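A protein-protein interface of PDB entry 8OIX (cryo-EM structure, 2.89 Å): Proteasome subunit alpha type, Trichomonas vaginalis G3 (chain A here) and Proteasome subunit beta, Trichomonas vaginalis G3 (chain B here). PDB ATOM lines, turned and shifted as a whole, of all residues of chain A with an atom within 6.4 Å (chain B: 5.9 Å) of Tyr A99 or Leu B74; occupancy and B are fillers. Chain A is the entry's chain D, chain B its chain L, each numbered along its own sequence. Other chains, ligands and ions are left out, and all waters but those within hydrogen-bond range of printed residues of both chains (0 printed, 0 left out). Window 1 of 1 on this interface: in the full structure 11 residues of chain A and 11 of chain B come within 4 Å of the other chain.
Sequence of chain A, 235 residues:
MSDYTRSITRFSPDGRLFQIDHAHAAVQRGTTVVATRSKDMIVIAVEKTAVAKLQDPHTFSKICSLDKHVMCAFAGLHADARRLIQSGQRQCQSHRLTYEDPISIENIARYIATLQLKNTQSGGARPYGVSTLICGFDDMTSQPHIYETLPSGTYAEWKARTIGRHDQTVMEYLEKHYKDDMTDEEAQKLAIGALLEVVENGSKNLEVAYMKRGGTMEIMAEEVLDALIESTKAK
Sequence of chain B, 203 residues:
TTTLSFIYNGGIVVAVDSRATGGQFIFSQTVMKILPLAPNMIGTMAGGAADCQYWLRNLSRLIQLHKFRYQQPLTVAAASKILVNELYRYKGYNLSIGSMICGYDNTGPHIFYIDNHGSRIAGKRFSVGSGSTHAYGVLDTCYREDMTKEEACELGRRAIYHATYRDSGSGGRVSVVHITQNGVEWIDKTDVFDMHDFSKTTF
Tyr A99 touches just these residues of chain B: Leu B74, Ala B77, Ala B78, Lys B81 and Ile B82. Ile B63 touches none of the printed residues of chain A. Gln B72 touches none of the printed residues of chain A. Of chain A, only Tyr A99 (3.7 Å) comes within 4 Å of Leu B74. Of the printed residues of chain A, Thr B75 touches Asp A101 (2.6 Å). Of the printed residues of chain A, Ile B82 touches Thr A98 (3.3 Å) and Tyr A99 (3.4 Å). The nearest residue of chain B that does not touch Tyr A99 is His B66 (4.4 Å). The nearest residue of chain A that does not touch Leu B74 is Asp A101 (6.0 Å). The nearest printed residue of chain A that does not touch Lys B81 is Arg A96 (4.4 Å).
Of the 21 printed residues of chain B, 8 touch a printed residue of chain A. Hydrophobic or aromatic side chains of chain B within 4 Å of the printed part of chain A: Leu B74, Ala B78 and Ile B82.
Among the printed residues, merely in contact across the chains: Tyr A99 with Ala B78, Thr A98 with Lys B81, Thr A98 with Asn B85, Tyr A99 with Ile B82, Tyr A99 with Lys B81, Asp A101 with Ala B78, Tyr A99 with Leu B74, Tyr A99 with Ala B77 and Glu A100 with Lys B81.
O of Leu A97 sits at hydrogen-bond distance from NZ of Lys B81 (2.8 Å). NH2 of Arg B120 lies within salt-bridge range of OE1 of Glu A100 (2.8 Å). The side-chain amide nitrogen (ND2) of Asn B85 is in hydrogen-bond range of the backbone carbonyl oxygen (O) of Leu A97, 2.7 Å away. The backbone NH of Ile B82 lies within hydrogen-bond range of the backbone carbonyl oxygen of Thr A98. The side-chain hydroxyl (OG1) of Thr B75 sits at hydrogen-bond distance from the side-chain carboxylate (OD2) of Asp A101, 2.6 Å away.
OG1 of Thr A98 is in hydrogen-bond range of O of Ser A94 (2.6 Å). The side-chain amino group (NZ) of Lys B81 is in hydrogen-bond range of the side-chain amide oxygen (OD1) of Asn B85 (2.5 Å). OG1 of Thr B75 is in hydrogen-bond range of N of Ala B78. The backbone carbonyl oxygen (O) of Ala B77 is in hydrogen-bond range of the guanidinium group (NH2) of Arg B120 (2.9 Å). O of Asp A101 lies within hydrogen-bond range of ND1 of His A95 (3.1 Å).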
ATOM      1  N   SER A  94     -21.842   4.690  18.157  1.00  0.00           N
ATOM      2  CA  SER A  94     -22.746   3.554  18.029  1.00  0.00           C
ATOM      3  C   SER A  94     -23.352   3.481  16.635  1.00  0.00           C
ATOM      4  O   SER A  94     -23.584   2.385  16.117  1.00  0.00           O
ATOM      5  CB  SER A  94     -23.843   3.636  19.089  1.00  0.00           C
ATOM      6  OG  SER A  94     -24.470   2.379  19.274  1.00  0.00           O
ATOM      7  N   HIS A  95     -23.620   4.631  16.019  1.00  0.00           N
ATOM      8  CA  HIS A  95     -24.072   4.656  14.635  1.00  0.00           C
ATOM      9  C   HIS A  95     -22.983   4.150  13.702  1.00  0.00           C
ATOM     10  O   HIS A  95     -23.272   3.459  12.722  1.00  0.00           O
ATOM     11  CB  HIS A  95     -24.500   6.072  14.253  1.00  0.00           C
ATOM     12  CG  HIS A  95     -25.205   6.159  12.936  1.00  0.00           C
ATOM     13  ND1 HIS A  95     -24.545   6.075  11.730  1.00  0.00           N
ATOM     14  CD2 HIS A  95     -26.514   6.325  12.636  1.00  0.00           C
ATOM     15  CE1 HIS A  95     -25.417   6.182  10.744  1.00  0.00           C
ATOM     16  NE2 HIS A  95     -26.620   6.335  11.268  1.00  0.00           N
ATOM     17  N   ARG A  96     -21.725   4.495  13.983  1.00  0.00           N
ATOM     18  CA  ARG A  96     -20.624   3.907  13.225  1.00  0.00           C
ATOM     19  C   ARG A  96     -20.557   2.396  13.430  1.00  0.00           C
ATOM     20  O   ARG A  96     -20.302   1.643  12.484  1.00  0.00           O
ATOM     21  CB  ARG A  96     -19.305   4.570  13.615  1.00  0.00           C
ATOM     22  CG  ARG A  96     -19.213   6.010  13.164  1.00  0.00           C
ATOM     23  CD  ARG A  96     -17.844   6.598  13.424  1.00  0.00           C
ATOM     24  NE  ARG A  96     -17.760   7.964  12.926  1.00  0.00           N
ATOM     25  CZ  ARG A  96     -17.508   8.283  11.665  1.00  0.00           C
ATOM     26  NH1 ARG A  96     -17.312   7.356  10.744  1.00  0.00           N
ATOM     27  NH2 ARG A  96     -17.462   9.565  11.317  1.00  0.00           N
ATOM     28  N   LEU A  97     -20.768   1.936  14.664  1.00  0.00           N
ATOM     29  CA  LEU A  97     -20.747   0.503  14.940  1.00  0.00           C
ATOM     30  C   LEU A  97     -21.858  -0.223  14.196  1.00  0.00           C
ATOM     31  O   LEU A  97     -21.651  -1.320  13.664  1.00  0.00           O
ATOM     32  CB  LEU A  97     -20.886   0.262  16.443  1.00  0.00           C
ATOM     33  CG  LEU A  97     -19.698   0.598  17.336  1.00  0.00           C
ATOM     34  CD1 LEU A  97     -20.132   0.687  18.787  1.00  0.00           C
ATOM     35  CD2 LEU A  97     -18.659  -0.475  17.171  1.00  0.00           C
ATOM     36  N   THR A  98     -23.047   0.372  14.158  1.00  0.00           N
ATOM     37  CA  THR A  98     -24.226  -0.273  13.599  1.00  0.00           C
ATOM     38  C   THR A  98     -24.326  -0.125  12.086  1.00  0.00           C
ATOM     39  O   THR A  98     -24.968  -0.958  11.438  1.00  0.00           O
ATOM     40  CB  THR A  98     -25.477   0.302  14.266  1.00  0.00           C
ATOM     41  OG1 THR A  98     -25.246   0.431  15.674  1.00  0.00           O
ATOM     42  CG2 THR A  98     -26.650  -0.622  14.072  1.00  0.00           C
ATOM     43  N   TYR A  99     -23.704   0.902  11.508  1.00  0.00           N
ATOM     44  CA  TYR A  99     -23.855   1.206  10.091  1.00  0.00           C
ATOM     45  C   TYR A  99     -22.544   1.391   9.339  1.00  0.00           C
ATOM     46  O   TYR A  99     -22.545   1.237   8.112  1.00  0.00           O
ATOM     47  CB  TYR A  99     -24.695   2.480   9.911  1.00  0.00           C
ATOM     48  CG  TYR A  99     -26.046   2.443  10.590  1.00  0.00           C
ATOM     49  CD1 TYR A  99     -27.121   1.787  10.009  1.00  0.00           C
ATOM     50  CD2 TYR A  99     -26.244   3.060  11.818  1.00  0.00           C
ATOM     51  CE1 TYR A  99     -28.357   1.754  10.628  1.00  0.00           C
ATOM     52  CE2 TYR A  99     -27.474   3.029  12.445  1.00  0.00           C
ATOM     53  CZ  TYR A  99     -28.526   2.374  11.847  1.00  0.00           C
ATOM     54  OH  TYR A  99     -29.753   2.341  12.465  1.00  0.00           O
ATOM     55  N   GLU A 100     -21.449   1.750  10.016  1.00  0.00           N
ATOM     56  CA  GLU A 100     -20.142   2.040   9.427  1.00  0.00           C
ATOM     57  C   GLU A 100     -20.184   3.374   8.689  1.00  0.00           C
ATOM     58  O   GLU A 100     -19.151   3.888   8.248  1.00  0.00           O
ATOM     59  CB  GLU A 100     -19.662   0.920   8.494  1.00  0.00           C
ATOM     60  CG  GLU A 100     -18.188   1.037   8.123  1.00  0.00           C
ATOM     61  CD  GLU A 100     -17.808   0.206   6.920  1.00  0.00           C
ATOM     62  OE1 GLU A 100     -18.265  -0.948   6.827  1.00  0.00           O
ATOM     63  OE2 GLU A 100     -17.055   0.712   6.062  1.00  0.00           O
ATOM     64  N   ASP A 101     -21.368   3.955   8.575  1.00  0.00           N
ATOM     65  CA  ASP A 101     -21.420   5.259   7.943  1.00  0.00           C
ATOM     66  C   ASP A 101     -21.418   6.345   9.004  1.00  0.00           C
ATOM     67  O   ASP A 101     -21.960   6.143  10.097  1.00  0.00           O
ATOM     68  CB  ASP A 101     -22.673   5.398   7.078  1.00  0.00           C
ATOM     69  CG  ASP A 101     -22.703   4.407   5.931  1.00  0.00           C
ATOM     70  OD1 ASP A 101     -21.738   3.630   5.788  1.00  0.00           O
ATOM     71  OD2 ASP A 101     -23.695   4.408   5.171  1.00  0.00           O
ATOM     72  N   PRO A 102     -20.794   7.488   8.731  1.00  0.00           N
ATOM     73  CA  PRO A 102     -20.904   8.616   9.659  1.00  0.00           C
ATOM     74  C   PRO A 102     -22.365   8.971   9.885  1.00  0.00           C
ATOM     75  O   PRO A 102     -23.161   9.017   8.945  1.00  0.00           O
ATOM     76  CB  PRO A 102     -20.146   9.740   8.947  1.00  0.00           C
ATOM     77  CG  PRO A 102     -19.222   9.043   8.010  1.00  0.00           C
ATOM     78  CD  PRO A 102     -19.931   7.797   7.579  1.00  0.00           C
ATOM     79  N   ASN A 107     -29.670  12.879  11.704  1.00  0.00           N
ATOM     80  CA  ASN A 107     -29.834  11.749  12.613  1.00  0.00           C
ATOM     81  C   ASN A 107     -29.324  12.084  14.012  1.00  0.00           C
ATOM     82  O   ASN A 107     -30.008  11.835  15.010  1.00  0.00           O
ATOM     83  CB  ASN A 107     -29.113  10.524  12.044  1.00  0.00           C
ATOM     84  CG  ASN A 107     -29.444   9.237  12.786  1.00  0.00           C
ATOM     85  OD1 ASN A 107     -29.747   9.243  13.979  1.00  0.00           O
ATOM     86  ND2 ASN A 107     -29.388   8.121  12.071  1.00  0.00           N
ATOM     87  N   ALA B  38     -34.225  -2.992  -0.582  1.00  0.00           N
ATOM     88  CA  ALA B  38     -34.555  -1.616  -0.916  1.00  0.00           C
ATOM     89  C   ALA B  38     -34.855  -1.559  -2.403  1.00  0.00           C
ATOM     90  O   ALA B  38     -34.561  -2.508  -3.138  1.00  0.00           O
ATOM     91  CB  ALA B  38     -33.386  -0.685  -0.550  1.00  0.00           C
ATOM     92  N   MET B  41     -31.655  -2.397  -3.756  1.00  0.00           N
ATOM     93  CA  MET B  41     -30.833  -3.277  -2.937  1.00  0.00           C
ATOM     94  C   MET B  41     -31.539  -4.608  -2.741  1.00  0.00           C
ATOM     95  O   MET B  41     -32.744  -4.637  -2.479  1.00  0.00           O
ATOM     96  CB  MET B  41     -30.551  -2.650  -1.570  1.00  0.00           C
ATOM     97  CG  MET B  41     -29.418  -3.285  -0.797  1.00  0.00           C
ATOM     98  SD  MET B  41     -29.377  -2.645   0.881  1.00  0.00           S
ATOM     99  CE  MET B  41     -29.384  -0.883   0.569  1.00  0.00           C
ATOM    100  N   LEU B  59     -33.993  -7.214   7.837  1.00  0.00           N
ATOM    101  CA  LEU B  59     -33.164  -6.141   7.302  1.00  0.00           C
ATOM    102  C   LEU B  59     -33.967  -5.229   6.387  1.00  0.00           C
ATOM    103  O   LEU B  59     -33.750  -4.016   6.370  1.00  0.00           O
ATOM    104  CB  LEU B  59     -31.959  -6.728   6.569  1.00  0.00           C
ATOM    105  CG  LEU B  59     -31.042  -5.719   5.887  1.00  0.00           C
ATOM    106  CD1 LEU B  59     -30.412  -4.827   6.922  1.00  0.00           C
ATOM    107  CD2 LEU B  59     -29.973  -6.438   5.096  1.00  0.00           C
ATOM    108  N   LEU B  62     -35.833  -3.008   8.706  1.00  0.00           N
ATOM    109  CA  LEU B  62     -34.950  -1.995   9.279  1.00  0.00           C
ATOM    110  C   LEU B  62     -34.583  -0.924   8.257  1.00  0.00           C
ATOM    111  O   LEU B  62     -34.490   0.260   8.601  1.00  0.00           O
ATOM    112  CB  LEU B  62     -33.704  -2.657   9.858  1.00  0.00           C
ATOM    113  CG  LEU B  62     -34.017  -3.551  11.059  1.00  0.00           C
ATOM    114  CD1 LEU B  62     -32.830  -4.408  11.449  1.00  0.00           C
ATOM    115  CD2 LEU B  62     -34.473  -2.702  12.235  1.00  0.00           C
ATOM    116  N   ILE B  63     -34.366  -1.315   6.999  1.00  0.00           N
ATOM    117  CA  ILE B  63     -34.061  -0.340   5.956  1.00  0.00           C
ATOM    118  C   ILE B  63     -35.244   0.590   5.735  1.00  0.00           C
ATOM    119  O   ILE B  63     -35.077   1.808   5.598  1.00  0.00           O
ATOM    120  CB  ILE B  63     -33.652  -1.054   4.653  1.00  0.00           C
ATOM    121  CG1 ILE B  63     -32.306  -1.756   4.822  1.00  0.00           C
ATOM    122  CG2 ILE B  63     -33.589  -0.070   3.495  1.00  0.00           C
ATOM    123  CD1 ILE B  63     -32.061  -2.829   3.796  1.00  0.00           C
ATOM    124  N   HIS B  66     -35.443   2.982   8.627  1.00  0.00           N
ATOM    125  CA  HIS B  66     -34.444   4.039   8.534  1.00  0.00           C
ATOM    126  C   HIS B  66     -34.810   5.060   7.464  1.00  0.00           C
ATOM    127  O   HIS B  66     -34.622   6.265   7.662  1.00  0.00           O
ATOM    128  CB  HIS B  66     -33.067   3.444   8.252  1.00  0.00           C
ATOM    129  CG  HIS B  66     -31.974   4.464   8.197  1.00  0.00           C
ATOM    130  ND1 HIS B  66     -31.610   5.102   7.031  1.00  0.00           N
ATOM    131  CD2 HIS B  66     -31.167   4.958   9.164  1.00  0.00           C
ATOM    132  CE1 HIS B  66     -30.625   5.945   7.282  1.00  0.00           C
ATOM    133  NE2 HIS B  66     -30.337   5.877   8.569  1.00  0.00           N
ATOM    134  N   LYS B  67     -35.324   4.601   6.321  1.00  0.00           N
ATOM    135  CA  LYS B  67     -35.691   5.536   5.261  1.00  0.00           C
ATOM    136  C   LYS B  67     -36.854   6.424   5.684  1.00  0.00           C
ATOM    137  O   LYS B  67     -36.921   7.593   5.289  1.00  0.00           O
ATOM    138  CB  LYS B  67     -36.012   4.788   3.964  1.00  0.00           C
ATOM    139  CG  LYS B  67     -37.396   4.176   3.884  1.00  0.00           C
ATOM    140  CD  LYS B  67     -37.852   4.014   2.446  1.00  0.00           C
ATOM    141  CE  LYS B  67     -38.266   5.345   1.849  1.00  0.00           C
ATOM    142  NZ  LYS B  67     -39.081   5.165   0.617  1.00  0.00           N
ATOM    143  N   ARG B  69     -37.656   7.142   8.982  1.00  0.00           N
ATOM    144  CA  ARG B  69     -37.132   7.987  10.052  1.00  0.00           C
ATOM    145  C   ARG B  69     -36.294   9.126   9.490  1.00  0.00           C
ATOM    146  O   ARG B  69     -36.438  10.282   9.902  1.00  0.00           O
ATOM    147  CB  ARG B  69     -36.294   7.151  11.019  1.00  0.00           C
ATOM    148  CG  ARG B  69     -37.068   6.227  11.935  1.00  0.00           C
ATOM    149  CD  ARG B  69     -36.106   5.255  12.593  1.00  0.00           C
ATOM    150  NE  ARG B  69     -36.727   4.450  13.637  1.00  0.00           N
ATOM    151  CZ  ARG B  69     -36.217   3.319  14.103  1.00  0.00           C
ATOM    152  NH1 ARG B  69     -35.093   2.817  13.618  1.00  0.00           N
ATOM    153  NH2 ARG B  69     -36.851   2.674  15.077  1.00  0.00           N
ATOM    154  N   GLN B  72     -32.789  10.302   3.921  1.00  0.00           N
ATOM    155  CA  GLN B  72     -31.754   9.569   3.208  1.00  0.00           C
ATOM    156  C   GLN B  72     -31.976   8.068   3.378  1.00  0.00           C
ATOM    157  O   GLN B  72     -32.142   7.594   4.510  1.00  0.00           O
ATOM    158  CB  GLN B  72     -30.371   9.969   3.722  1.00  0.00           C
ATOM    159  CG  GLN B  72     -30.256   9.995   5.238  1.00  0.00           C
ATOM    160  CD  GLN B  72     -30.498  11.376   5.816  1.00  0.00           C
ATOM    161  OE1 GLN B  72     -30.760  12.330   5.083  1.00  0.00           O
ATOM    162  NE2 GLN B  72     -30.422  11.487   7.136  1.00  0.00           N
ATOM    163  N   PRO B  73     -32.002   7.297   2.295  1.00  0.00           N
ATOM    164  CA  PRO B  73     -32.177   5.848   2.427  1.00  0.00           C
ATOM    165  C   PRO B  73     -30.944   5.197   3.030  1.00  0.00           C
ATOM    166  O   PRO B  73     -29.829   5.719   2.965  1.00  0.00           O
ATOM    167  CB  PRO B  73     -32.407   5.370   0.986  1.00  0.00           C
ATOM    168  CG  PRO B  73     -32.420   6.599   0.126  1.00  0.00           C
ATOM    169  CD  PRO B  73     -31.803   7.713   0.898  1.00  0.00           C
ATOM    170  N   LEU B  74     -31.164   4.030   3.630  1.00  0.00           N
ATOM    171  CA  LEU B  74     -30.065   3.289   4.229  1.00  0.00           C
ATOM    172  C   LEU B  74     -29.172   2.732   3.130  1.00  0.00           C
ATOM    173  O   LEU B  74     -29.650   2.068   2.206  1.00  0.00           O
ATOM    174  CB  LEU B  74     -30.607   2.162   5.106  1.00  0.00           C
ATOM    175  CG  LEU B  74     -29.684   1.606   6.189  1.00  0.00           C
ATOM    176  CD1 LEU B  74     -29.155   2.735   7.052  1.00  0.00           C
ATOM    177  CD2 LEU B  74     -30.414   0.581   7.037  1.00  0.00           C
ATOM    178  N   THR B  75     -27.873   3.005   3.225  1.00  0.00           N
ATOM    179  CA  THR B  75     -26.957   2.602   2.172  1.00  0.00           C
ATOM    180  C   THR B  75     -26.738   1.091   2.204  1.00  0.00           C
ATOM    181  O   THR B  75     -27.185   0.386   3.111  1.00  0.00           O
ATOM    182  CB  THR B  75     -25.620   3.331   2.307  1.00  0.00           C
ATOM    183  OG1 THR B  75     -24.931   2.865   3.472  1.00  0.00           O
ATOM    184  CG2 THR B  75     -25.845   4.829   2.427  1.00  0.00           C
ATOM    185  N   VAL B  76     -26.034   0.595   1.186  1.00  0.00           N
ATOM    186  CA  VAL B  76     -25.778  -0.837   1.104  1.00  0.00           C
ATOM    187  C   VAL B  76     -24.759  -1.254   2.150  1.00  0.00           C
ATOM    188  O   VAL B  76     -24.884  -2.325   2.761  1.00  0.00           O
ATOM    189  CB  VAL B  76     -25.312  -1.203  -0.314  1.00  0.00           C
ATOM    190  CG1 VAL B  76     -25.154  -2.711  -0.455  1.00  0.00           C
ATOM    191  CG2 VAL B  76     -26.274  -0.641  -1.336  1.00  0.00           C
ATOM    192  N   ALA B  77     -23.762  -0.408   2.405  1.00  0.00           N
ATOM    193  CA  ALA B  77     -22.819  -0.680   3.481  1.00  0.00           C
ATOM    194  C   ALA B  77     -23.516  -0.644   4.832  1.00  0.00           C
ATOM    195  O   ALA B  77     -23.312  -1.526   5.671  1.00  0.00           O
ATOM    196  CB  ALA B  77     -21.669   0.326   3.438  1.00  0.00           C
ATOM    197  N   ALA B  78     -24.362   0.366   5.053  1.00  0.00           N
ATOM    198  CA  ALA B  78     -25.081   0.465   6.318  1.00  0.00           C
ATOM    199  C   ALA B  78     -26.049  -0.697   6.504  1.00  0.00           C
ATOM    200  O   ALA B  78     -26.185  -1.228   7.611  1.00  0.00           O
ATOM    201  CB  ALA B  78     -25.816   1.801   6.396  1.00  0.00           C
ATOM    202  N   ALA B  79     -26.741  -1.098   5.436  1.00  0.00           N
ATOM    203  CA  ALA B  79     -27.670  -2.219   5.535  1.00  0.00           C
ATOM    204  C   ALA B  79     -26.934  -3.516   5.842  1.00  0.00           C
ATOM    205  O   ALA B  79     -27.338  -4.283   6.727  1.00  0.00           O
ATOM    206  CB  ALA B  79     -28.474  -2.348   4.245  1.00  0.00           C
ATOM    207  N   LYS B  81     -24.146  -3.751   7.280  1.00  0.00           N
ATOM    208  CA  LYS B  81     -23.626  -3.619   8.634  1.00  0.00           C
ATOM    209  C   LYS B  81     -24.696  -3.940   9.668  1.00  0.00           C
ATOM    210  O   LYS B  81     -24.426  -4.633  10.655  1.00  0.00           O
ATOM    211  CB  LYS B  81     -23.094  -2.204   8.835  1.00  0.00           C
ATOM    212  CG  LYS B  81     -22.245  -2.036  10.059  1.00  0.00           C
ATOM    213  CD  LYS B  81     -20.921  -2.723   9.878  1.00  0.00           C
ATOM    214  CE  LYS B  81     -20.077  -2.544  11.107  1.00  0.00           C
ATOM    215  NZ  LYS B  81     -20.530  -3.425  12.218  1.00  0.00           N
ATOM    216  N   ILE B  82     -25.912  -3.432   9.461  1.00  0.00           N
ATOM    217  CA  ILE B  82     -27.033  -3.770  10.334  1.00  0.00           C
ATOM    218  C   ILE B  82     -27.222  -5.278  10.379  1.00  0.00           C
ATOM    219  O   ILE B  82     -27.319  -5.885  11.456  1.00  0.00           O
ATOM    220  CB  ILE B  82     -28.314  -3.066   9.847  1.00  0.00           C
ATOM    221  CG1 ILE B  82     -28.416  -1.653  10.413  1.00  0.00           C
ATOM    222  CG2 ILE B  82     -29.541  -3.867  10.240  1.00  0.00           C
ATOM    223  CD1 ILE B  82     -29.052  -1.596  11.780  1.00  0.00           C
ATOM    224  N   ASN B  85     -24.270  -7.096  12.173  1.00  0.00           N
ATOM    225  CA  ASN B  85     -24.311  -6.902  13.620  1.00  0.00           C
ATOM    226  C   ASN B  85     -25.399  -7.759  14.253  1.00  0.00           C
ATOM    227  O   ASN B  85     -25.172  -8.418  15.278  1.00  0.00           O
ATOM    228  CB  ASN B  85     -24.525  -5.425  13.945  1.00  0.00           C
ATOM    229  CG  ASN B  85     -23.314  -4.579  13.622  1.00  0.00           C
ATOM    230  OD1 ASN B  85     -22.493  -4.945  12.785  1.00  0.00           O
ATOM    231  ND2 ASN B  85     -23.195  -3.437  14.289  1.00  0.00           N
ATOM    232  N   ASP B 105     -26.013   2.253  -4.222  1.00  0.00           N
ATOM    233  CA  ASP B 105     -26.292   3.374  -3.334  1.00  0.00           C
ATOM    234  C   ASP B 105     -25.678   4.653  -3.887  1.00  0.00           C
ATOM    235  O   ASP B 105     -25.241   4.691  -5.042  1.00  0.00           O
ATOM    236  CB  ASP B 105     -25.783   3.090  -1.919  1.00  0.00           C
ATOM    237  CG  ASP B 105     -24.315   2.722  -1.886  1.00  0.00           C
ATOM    238  OD1 ASP B 105     -23.944   1.691  -2.480  1.00  0.00           O
ATOM    239  OD2 ASP B 105     -23.532   3.463  -1.257  1.00  0.00           O
ATOM    240  N   ARG B 120     -18.217  -9.464   7.196  1.00  0.00           N
ATOM    241  CA  ARG B 120     -18.851  -8.494   6.302  1.00  0.00           C
ATOM    242  C   ARG B 120     -17.760  -8.004   5.355  1.00  0.00           C
ATOM    243  O   ARG B 120     -17.028  -7.060   5.664  1.00  0.00           O
ATOM    244  CB  ARG B 120     -19.486  -7.354   7.082  1.00  0.00           C
ATOM    245  CG  ARG B 120     -19.990  -6.219   6.221  1.00  0.00           C
ATOM    246  CD  ARG B 120     -20.764  -5.229   7.055  1.00  0.00           C
ATOM    247  NE  ARG B 120     -21.015  -3.994   6.327  1.00  0.00           N
ATOM    248  CZ  ARG B 120     -20.108  -3.050   6.131  1.00  0.00           C
ATOM    249  NH1 ARG B 120     -18.871  -3.176   6.577  1.00  0.00           N
ATOM    250  NH2 ARG B 120     -20.451  -1.950   5.468  1.00  0.00           N
